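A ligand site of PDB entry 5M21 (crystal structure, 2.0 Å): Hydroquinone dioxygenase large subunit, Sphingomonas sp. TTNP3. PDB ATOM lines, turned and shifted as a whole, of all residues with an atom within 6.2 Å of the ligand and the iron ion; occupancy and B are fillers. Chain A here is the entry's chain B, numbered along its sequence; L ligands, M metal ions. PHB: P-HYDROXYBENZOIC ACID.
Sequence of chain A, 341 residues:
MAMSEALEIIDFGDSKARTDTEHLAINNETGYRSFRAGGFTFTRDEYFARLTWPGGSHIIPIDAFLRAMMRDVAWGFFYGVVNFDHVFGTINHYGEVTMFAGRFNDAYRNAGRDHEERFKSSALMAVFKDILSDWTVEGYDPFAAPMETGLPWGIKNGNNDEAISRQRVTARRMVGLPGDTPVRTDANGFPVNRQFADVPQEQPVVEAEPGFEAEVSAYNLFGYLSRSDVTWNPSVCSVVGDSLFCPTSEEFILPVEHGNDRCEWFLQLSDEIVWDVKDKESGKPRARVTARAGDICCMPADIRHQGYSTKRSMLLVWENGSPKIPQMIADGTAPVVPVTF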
ATOM      1  N   TRP A  75      26.221  -1.706   7.055  1.00  0.00           N
ATOM      2  CA  TRP A  75      25.481  -2.690   6.246  1.00  0.00           C
ATOM      3  C   TRP A  75      25.984  -2.795   4.819  1.00  0.00           C
ATOM      4  O   TRP A  75      25.346  -3.491   3.996  1.00  0.00           O
ATOM      5  CB  TRP A  75      23.959  -2.409   6.215  1.00  0.00           C
ATOM      6  CG  TRP A  75      23.265  -2.189   7.523  1.00  0.00           C
ATOM      7  CD1 TRP A  75      23.627  -2.695   8.772  1.00  0.00           C
ATOM      8  CD2 TRP A  75      22.023  -1.499   7.730  1.00  0.00           C
ATOM      9  NE1 TRP A  75      22.713  -2.302   9.725  1.00  0.00           N
ATOM     10  CE2 TRP A  75      21.710  -1.590   9.118  1.00  0.00           C
ATOM     11  CE3 TRP A  75      21.176  -0.752   6.887  1.00  0.00           C
ATOM     12  CZ2 TRP A  75      20.581  -0.970   9.682  1.00  0.00           C
ATOM     13  CZ3 TRP A  75      20.038  -0.135   7.453  1.00  0.00           C
ATOM     14  CH2 TRP A  75      19.770  -0.223   8.851  1.00  0.00           C
ATOM     15  N   PHE A  78      23.191  -2.078   2.569  1.00  0.00           N
ATOM     16  CA  PHE A  78      22.045  -2.946   2.880  1.00  0.00           C
ATOM     17  C   PHE A  78      21.355  -3.519   1.618  1.00  0.00           C
ATOM     18  O   PHE A  78      22.033  -3.850   0.654  1.00  0.00           O
ATOM     19  CB  PHE A  78      21.074  -2.125   3.693  1.00  0.00           C
ATOM     20  CG  PHE A  78      20.291  -2.929   4.660  1.00  0.00           C
ATOM     21  CD1 PHE A  78      20.842  -4.079   5.259  1.00  0.00           C
ATOM     22  CD2 PHE A  78      19.010  -2.522   5.034  1.00  0.00           C
ATOM     23  CE1 PHE A  78      20.118  -4.838   6.175  1.00  0.00           C
ATOM     24  CE2 PHE A  78      18.283  -3.272   5.952  1.00  0.00           C
ATOM     25  CZ  PHE A  78      18.830  -4.427   6.520  1.00  0.00           C
ATOM     26  N   THR A 231      22.679  -1.234  18.234  1.00  0.00           N
ATOM     27  CA  THR A 231      21.240  -1.214  18.100  1.00  0.00           C
ATOM     28  C   THR A 231      20.930  -1.240  16.610  1.00  0.00           C
ATOM     29  O   THR A 231      21.742  -0.734  15.789  1.00  0.00           O
ATOM     30  CB  THR A 231      20.592  -0.009  18.780  1.00  0.00           C
ATOM     31  OG1 THR A 231      21.107   1.234  18.213  1.00  0.00           O
ATOM     32  CG2 THR A 231      20.909  -0.041  20.249  1.00  0.00           C
ATOM     33  N   TRP A 232      19.810  -1.820  16.225  1.00  0.00           N
ATOM     34  CA  TRP A 232      19.390  -1.750  14.810  1.00  0.00           C
ATOM     35  C   TRP A 232      20.477  -2.223  13.851  1.00  0.00           C
ATOM     36  O   TRP A 232      20.928  -1.479  12.964  1.00  0.00           O
ATOM     37  CB  TRP A 232      18.921  -0.379  14.401  1.00  0.00           C
ATOM     38  CG  TRP A 232      17.907   0.178  15.343  1.00  0.00           C
ATOM     39  CD1 TRP A 232      18.125   1.101  16.324  1.00  0.00           C
ATOM     40  CD2 TRP A 232      16.478  -0.115  15.346  1.00  0.00           C
ATOM     41  NE1 TRP A 232      16.912   1.432  16.929  1.00  0.00           N
ATOM     42  CE2 TRP A 232      15.895   0.693  16.367  1.00  0.00           C
ATOM     43  CE3 TRP A 232      15.659  -0.978  14.598  1.00  0.00           C
ATOM     44  CZ2 TRP A 232      14.516   0.633  16.686  1.00  0.00           C
ATOM     45  CZ3 TRP A 232      14.287  -1.017  14.886  1.00  0.00           C
ATOM     46  CH2 TRP A 232      13.727  -0.221  15.942  1.00  0.00           C
ATOM     47  N   ASN A 233      20.849  -3.488  13.999  1.00  0.00           N
ATOM     48  CA  ASN A 233      21.916  -4.066  13.218  1.00  0.00           C
ATOM     49  C   ASN A 233      21.695  -5.568  12.956  1.00  0.00           C
ATOM     50  O   ASN A 233      22.260  -6.424  13.659  1.00  0.00           O
ATOM     51  CB  ASN A 233      23.280  -3.816  13.874  1.00  0.00           C
ATOM     52  CG  ASN A 233      24.410  -4.098  12.911  1.00  0.00           C
ATOM     53  OD1 ASN A 233      24.377  -3.661  11.742  1.00  0.00           O
ATOM     54  ND2 ASN A 233      25.403  -4.840  13.360  1.00  0.00           N
ATOM     55  N   PRO A 234      20.810  -5.889  11.983  1.00  0.00           N
ATOM     56  CA  PRO A 234      20.478  -7.252  11.614  1.00  0.00           C
ATOM     57  C   PRO A 234      21.783  -7.991  11.299  1.00  0.00           C
ATOM     58  O   PRO A 234      22.618  -7.496  10.513  1.00  0.00           O
ATOM     59  CB  PRO A 234      19.698  -7.075  10.312  1.00  0.00           C
ATOM     60  CG  PRO A 234      19.117  -5.704  10.414  1.00  0.00           C
ATOM     61  CD  PRO A 234      20.219  -4.922  11.053  1.00  0.00           C
ATOM     62  N   THR A 248      18.594  -8.928  15.904  1.00  0.00           N
ATOM     63  CA  THR A 248      19.285  -7.709  16.353  1.00  0.00           C
ATOM     64  C   THR A 248      18.544  -7.200  17.570  1.00  0.00           C
ATOM     65  O   THR A 248      17.357  -7.579  17.779  1.00  0.00           O
ATOM     66  CB  THR A 248      19.280  -6.608  15.224  1.00  0.00           C
ATOM     67  OG1 THR A 248      19.690  -5.340  15.735  1.00  0.00           O
ATOM     68  CG2 THR A 248      17.877  -6.429  14.622  1.00  0.00           C
ATOM     69  N   SER A 249      19.219  -6.405  18.389  1.00  0.00           N
ATOM     70  CA  SER A 249      18.513  -5.698  19.470  1.00  0.00           C
ATOM     71  C   SER A 249      18.274  -4.225  19.150  1.00  0.00           C
ATOM     72  O   SER A 249      19.198  -3.494  18.772  1.00  0.00           O
ATOM     73  CB  SER A 249      19.239  -5.836  20.803  1.00  0.00           C
ATOM     74  OG  SER A 249      20.533  -5.245  20.723  1.00  0.00           O
ATOM     75  N   GLU A 250      17.061  -3.768  19.418  1.00  0.00           N
ATOM     76  CA  GLU A 250      16.569  -2.507  18.894  1.00  0.00           C
ATOM     77  C   GLU A 250      16.227  -1.556  20.029  1.00  0.00           C
ATOM     78  O   GLU A 250      15.543  -1.929  20.930  1.00  0.00           O
ATOM     79  CB  GLU A 250      15.272  -2.761  18.125  1.00  0.00           C
ATOM     80  CG  GLU A 250      15.238  -3.980  17.196  1.00  0.00           C
ATOM     81  CD  GLU A 250      16.252  -3.909  16.088  1.00  0.00           C
ATOM     82  OE1 GLU A 250      17.450  -3.706  16.436  1.00  0.00           O
ATOM     83  OE2 GLU A 250      15.891  -4.051  14.866  1.00  0.00           O
ATOM     84  N   LEU A 254      14.882   3.272  14.602  1.00  0.00           N
ATOM     85  CA  LEU A 254      15.657   2.854  13.463  1.00  0.00           C
ATOM     86  C   LEU A 254      16.134   4.118  12.752  1.00  0.00           C
ATOM     87  O   LEU A 254      15.325   4.923  12.306  1.00  0.00           O
ATOM     88  CB  LEU A 254      14.816   1.991  12.501  1.00  0.00           C
ATOM     89  CG  LEU A 254      15.560   1.544  11.261  1.00  0.00           C
ATOM     90  CD1 LEU A 254      16.829   0.810  11.626  1.00  0.00           C
ATOM     91  CD2 LEU A 254      14.684   0.583  10.471  1.00  0.00           C
ATOM     92  N   VAL A 256      17.100   4.844   9.925  1.00  0.00           N
ATOM     93  CA  VAL A 256      16.744   5.048   8.492  1.00  0.00           C
ATOM     94  C   VAL A 256      15.281   4.646   8.227  1.00  0.00           C
ATOM     95  O   VAL A 256      14.687   4.016   9.065  1.00  0.00           O
ATOM     96  CB  VAL A 256      17.699   4.261   7.563  1.00  0.00           C
ATOM     97  CG1 VAL A 256      19.163   4.648   7.805  1.00  0.00           C
ATOM     98  CG2 VAL A 256      17.520   2.773   7.793  1.00  0.00           C
ATOM     99  N   HIS A 258      13.744   2.225   5.667  1.00  0.00           N
ATOM    100  CA  HIS A 258      14.170   1.199   4.738  1.00  0.00           C
ATOM    101  C   HIS A 258      13.077   0.922   3.692  1.00  0.00           C
ATOM    102  O   HIS A 258      12.002   0.472   4.037  1.00  0.00           O
ATOM    103  CB  HIS A 258      14.565  -0.085   5.484  1.00  0.00           C
ATOM    104  CG  HIS A 258      15.162  -1.113   4.583  1.00  0.00           C
ATOM    105  ND1 HIS A 258      15.024  -2.473   4.790  1.00  0.00           N
ATOM    106  CD2 HIS A 258      15.793  -0.980   3.388  1.00  0.00           C
ATOM    107  CE1 HIS A 258      15.584  -3.130   3.788  1.00  0.00           C
ATOM    108  NE2 HIS A 258      16.059  -2.242   2.926  1.00  0.00           N
ATOM    109  N   GLY A 259      13.392   1.148   2.417  1.00  0.00           N
ATOM    110  CA  GLY A 259      12.544   0.697   1.321  1.00  0.00           C
ATOM    111  C   GLY A 259      13.203  -0.474   0.601  1.00  0.00           C
ATOM    112  O   GLY A 259      14.114  -0.293  -0.212  1.00  0.00           O
ATOM    113  N   ASN A 260      12.773  -1.678   0.910  1.00  0.00           N
ATOM    114  CA  ASN A 260      13.508  -2.845   0.463  1.00  0.00           C
ATOM    115  C   ASN A 260      13.177  -3.072  -0.989  1.00  0.00           C
ATOM    116  O   ASN A 260      12.196  -2.505  -1.509  1.00  0.00           O
ATOM    117  CB  ASN A 260      13.237  -4.015   1.395  1.00  0.00           C
ATOM    118  CG  ASN A 260      14.352  -5.049   1.389  1.00  0.00           C
ATOM    119  OD1 ASN A 260      15.120  -5.127   0.450  1.00  0.00           O
ATOM    120  ND2 ASN A 260      14.402  -5.903   2.418  1.00  0.00           N
ATOM    121  N   GLU A 264      10.355  -8.544   3.040  1.00  0.00           N
ATOM    122  CA  GLU A 264      11.059  -8.979   4.219  1.00  0.00           C
ATOM    123  C   GLU A 264      10.092  -9.143   5.374  1.00  0.00           C
ATOM    124  O   GLU A 264       9.004  -8.596   5.361  1.00  0.00           O
ATOM    125  CB  GLU A 264      12.183  -7.988   4.570  1.00  0.00           C
ATOM    126  CG  GLU A 264      11.772  -6.802   5.404  1.00  0.00           C
ATOM    127  CD  GLU A 264      12.873  -5.785   5.482  1.00  0.00           C
ATOM    128  OE1 GLU A 264      13.845  -6.003   6.204  1.00  0.00           O
ATOM    129  OE2 GLU A 264      12.789  -4.799   4.755  1.00  0.00           O
ATOM    130  N   PHE A 266       9.462  -9.616   9.782  1.00  0.00           N
ATOM    131  CA  PHE A 266       9.896  -9.208  11.129  1.00  0.00           C
ATOM    132  C   PHE A 266       9.222 -10.116  12.103  1.00  0.00           C
ATOM    133  O   PHE A 266       7.962 -10.237  12.088  1.00  0.00           O
ATOM    134  CB  PHE A 266       9.397  -7.790  11.509  1.00  0.00           C
ATOM    135  CG  PHE A 266      10.042  -6.670  10.700  1.00  0.00           C
ATOM    136  CD1 PHE A 266      11.328  -6.811  10.177  1.00  0.00           C
ATOM    137  CD2 PHE A 266       9.352  -5.474  10.469  1.00  0.00           C
ATOM    138  CE1 PHE A 266      11.932  -5.768   9.441  1.00  0.00           C
ATOM    139  CE2 PHE A 266       9.950  -4.444   9.733  1.00  0.00           C
ATOM    140  CZ  PHE A 266      11.241  -4.587   9.229  1.00  0.00           C
ATOM    141  N   TRP A 275       6.052   0.001  13.950  1.00  0.00           N
ATOM    142  CA  TRP A 275       6.620   0.352  12.659  1.00  0.00           C
ATOM    143  C   TRP A 275       5.790   1.446  11.980  1.00  0.00           C
ATOM    144  O   TRP A 275       4.568   1.258  11.808  1.00  0.00           O
ATOM    145  CB  TRP A 275       6.663  -0.904  11.767  1.00  0.00           C
ATOM    146  CG  TRP A 275       7.575  -1.961  12.325  1.00  0.00           C
ATOM    147  CD1 TRP A 275       7.226  -3.045  13.102  1.00  0.00           C
ATOM    148  CD2 TRP A 275       8.999  -2.012  12.166  1.00  0.00           C
ATOM    149  NE1 TRP A 275       8.352  -3.774  13.422  1.00  0.00           N
ATOM    150  CE2 TRP A 275       9.459  -3.140  12.897  1.00  0.00           C
ATOM    151  CE3 TRP A 275       9.939  -1.188  11.516  1.00  0.00           C
ATOM    152  CZ2 TRP A 275      10.823  -3.497  12.970  1.00  0.00           C
ATOM    153  CZ3 TRP A 275      11.300  -1.544  11.579  1.00  0.00           C
ATOM    154  CH2 TRP A 275      11.724  -2.686  12.318  1.00  0.00           C
ATOM    155  N   MET A 299       6.879  -6.868   5.533  1.00  0.00           N
ATOM    156  CA  MET A 299       6.900  -5.537   4.923  1.00  0.00           C
ATOM    157  C   MET A 299       6.852  -5.706   3.414  1.00  0.00           C
ATOM    158  O   MET A 299       7.752  -6.259   2.827  1.00  0.00           O
ATOM    159  CB  MET A 299       8.170  -4.761   5.297  1.00  0.00           C
ATOM    160  CG  MET A 299       8.253  -4.570   6.810  1.00  0.00           C
ATOM    161  SD  MET A 299       7.131  -3.241   7.238  1.00  0.00           S
ATOM    162  CE  MET A 299       6.145  -4.030   8.524  1.00  0.00           C
ATOM    163  N   HIS A 305       9.927   1.580   5.744  1.00  0.00           N
ATOM    164  CA  HIS A 305       9.500   1.481   7.141  1.00  0.00           C
ATOM    165  C   HIS A 305      10.572   1.950   8.086  1.00  0.00           C
ATOM    166  O   HIS A 305      11.773   1.866   7.741  1.00  0.00           O
ATOM    167  CB  HIS A 305       9.179   0.046   7.480  1.00  0.00           C
ATOM    168  CG  HIS A 305      10.155  -0.916   6.895  1.00  0.00           C
ATOM    169  ND1 HIS A 305       9.980  -1.478   5.654  1.00  0.00           N
ATOM    170  CD2 HIS A 305      11.328  -1.383   7.368  1.00  0.00           C
ATOM    171  CE1 HIS A 305      11.014  -2.234   5.378  1.00  0.00           C
ATOM    172  NE2 HIS A 305      11.842  -2.207   6.405  1.00  0.00           N
ATOM    173  N   LEU A 315      14.583  -8.513  17.993  1.00  0.00           N
ATOM    174  CA  LEU A 315      13.795  -8.638  16.804  1.00  0.00           C
ATOM    175  C   LEU A 315      14.495  -9.635  15.880  1.00  0.00           C
ATOM    176  O   LEU A 315      15.700  -9.658  15.826  1.00  0.00           O
ATOM    177  CB  LEU A 315      13.724  -7.264  16.152  1.00  0.00           C
ATOM    178  CG  LEU A 315      13.134  -7.271  14.719  1.00  0.00           C
ATOM    179  CD1 LEU A 315      11.646  -7.530  14.765  1.00  0.00           C
ATOM    180  CD2 LEU A 315      13.397  -5.941  14.055  1.00  0.00           C
ATOM    181  N   VAL A 317      14.923 -10.259  11.978  1.00  0.00           N
ATOM    182  CA  VAL A 317      14.616  -9.745  10.641  1.00  0.00           C
ATOM    183  C   VAL A 317      14.877 -10.927   9.671  1.00  0.00           C
ATOM    184  O   VAL A 317      15.957 -11.447   9.648  1.00  0.00           O
ATOM    185  CB  VAL A 317      15.495  -8.528  10.297  1.00  0.00           C
ATOM    186  CG1 VAL A 317      15.218  -8.087   8.858  1.00  0.00           C
ATOM    187  CG2 VAL A 317      15.225  -7.380  11.265  1.00  0.00           C
ATOM    188  N   GLU A 319      15.259 -12.405   5.861  1.00  0.00           N
ATOM    189  CA  GLU A 319      15.587 -11.949   4.513  1.00  0.00           C
ATOM    190  C   GLU A 319      15.764 -13.124   3.524  1.00  0.00           C
ATOM    191  O   GLU A 319      16.234 -14.206   3.862  1.00  0.00           O
ATOM    192  CB  GLU A 319      16.905 -11.130   4.514  1.00  0.00           C
ATOM    193  CG  GLU A 319      16.881  -9.834   5.313  1.00  0.00           C
ATOM    194  CD  GLU A 319      16.206  -8.578   4.638  1.00  0.00           C
ATOM    195  OE1 GLU A 319      16.143  -7.550   5.365  1.00  0.00           O
ATOM    196  OE2 GLU A 319      15.795  -8.518   3.407  1.00  0.00           O
HETATM  197  C1' PHB L   1      14.938  -3.071   8.353  1.00  0.00           C
HETATM  198  O1' PHB L   1      14.038  -3.881   8.158  1.00  0.00           O
HETATM  199  O2' PHB L   1      15.423  -2.358   7.463  1.00  0.00           O
HETATM  200  C1  PHB L   1      15.581  -3.046   9.702  1.00  0.00           C
HETATM  201  C2  PHB L   1      15.022  -3.753  10.770  1.00  0.00           C
HETATM  202  C3  PHB L   1      15.697  -3.857  11.976  1.00  0.00           C
HETATM  203  C4  PHB L   1      16.949  -3.269  12.116  1.00  0.00           C
HETATM  204  C5  PHB L   1      17.502  -2.559  11.071  1.00  0.00           C
HETATM  205  C6  PHB L   1      16.820  -2.438   9.870  1.00  0.00           C
HETATM  206  O4  PHB L   1      17.645  -3.396  13.271  1.00  0.00           O
HETATM  207 FE    FE M   1      13.727  -3.372   6.215  1.00  0.00          FE
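The iron ion is bound by O1' of the ligand (2.0 Å), ND1 of His 258 (2.1 Å), NE2 of His 305 (2.2 Å), OE2 of Glu 264 (2.2 Å) and O2' of the ligand (2.3 Å). The iron ion has five donor atoms within binding distance. Slightly farther from the iron ion lies OE1 of Glu 264 (2.6 Å).
O4 of the ligand sits at hydrogen-bond distance from OE2 of Glu 250, at 2.5 Å. The backbone NH (N) of Asn 233 is in hydrogen-bond range of an oxygen (O4) of the ligand (3.3 Å).
Merely in contact with the ligand: Trp 232 (2.9 Å), Phe 266 (3.1 Å), Thr 248 (3.3 Å), Phe 78 (3.4 Å), Leu 254 (3.5 Å), Pro 234 (3.6 Å), Val 317 (3.6 Å), Trp 75 (3.7 Å), Leu 315 (3.7 Å) and Trp 275 (3.8 Å). Hydrophobic or aromatic side chains within 4 Å of the ligand: Trp 75, Phe 78, Trp 232, Pro 234, Leu 254, His 258, Phe 266, Trp 275, His 305, Leu 315 and Val 317. The nearest printed residue that does not touch the ligand is Glu 319 (5.1 Å).
N of Asn 233 lies within hydrogen-bond range of OG1 of Thr 248 (2.8 Å). The side-chain carboxylate of Glu 250 is in hydrogen-bond range of the backbone NH of Trp 232 (3.0 Å). The backbone carbonyl oxygen (O) of Ser 249 sits at hydrogen-bond distance from the backbone NH (N) of Trp 232. NE1 of Trp 75 is in hydrogen-bond range of OD1 of Asn 233 (2.9 Å). The side-chain carboxylate (OE2) of Glu 264 sits close to the side-chain amide nitrogen (ND2) of Asn 260, 3.0 Å away. OE1 of Glu 250 is in hydrogen-bond range of OG1 of Thr 248 (2.9 Å). The backbone carbonyl oxygen (O) of Glu 264 lies within hydrogen-bond range of the backbone NH (N) of Met 299 (2.7 Å). N of Leu 315 lies within hydrogen-bond range of O of Thr 248 (2.9 Å).
Of the 22 residues printed, 3 come within 4 Å of the iron ion. The nearest printed residue that does not touch the iron ion is Phe 266 (4.1 Å).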
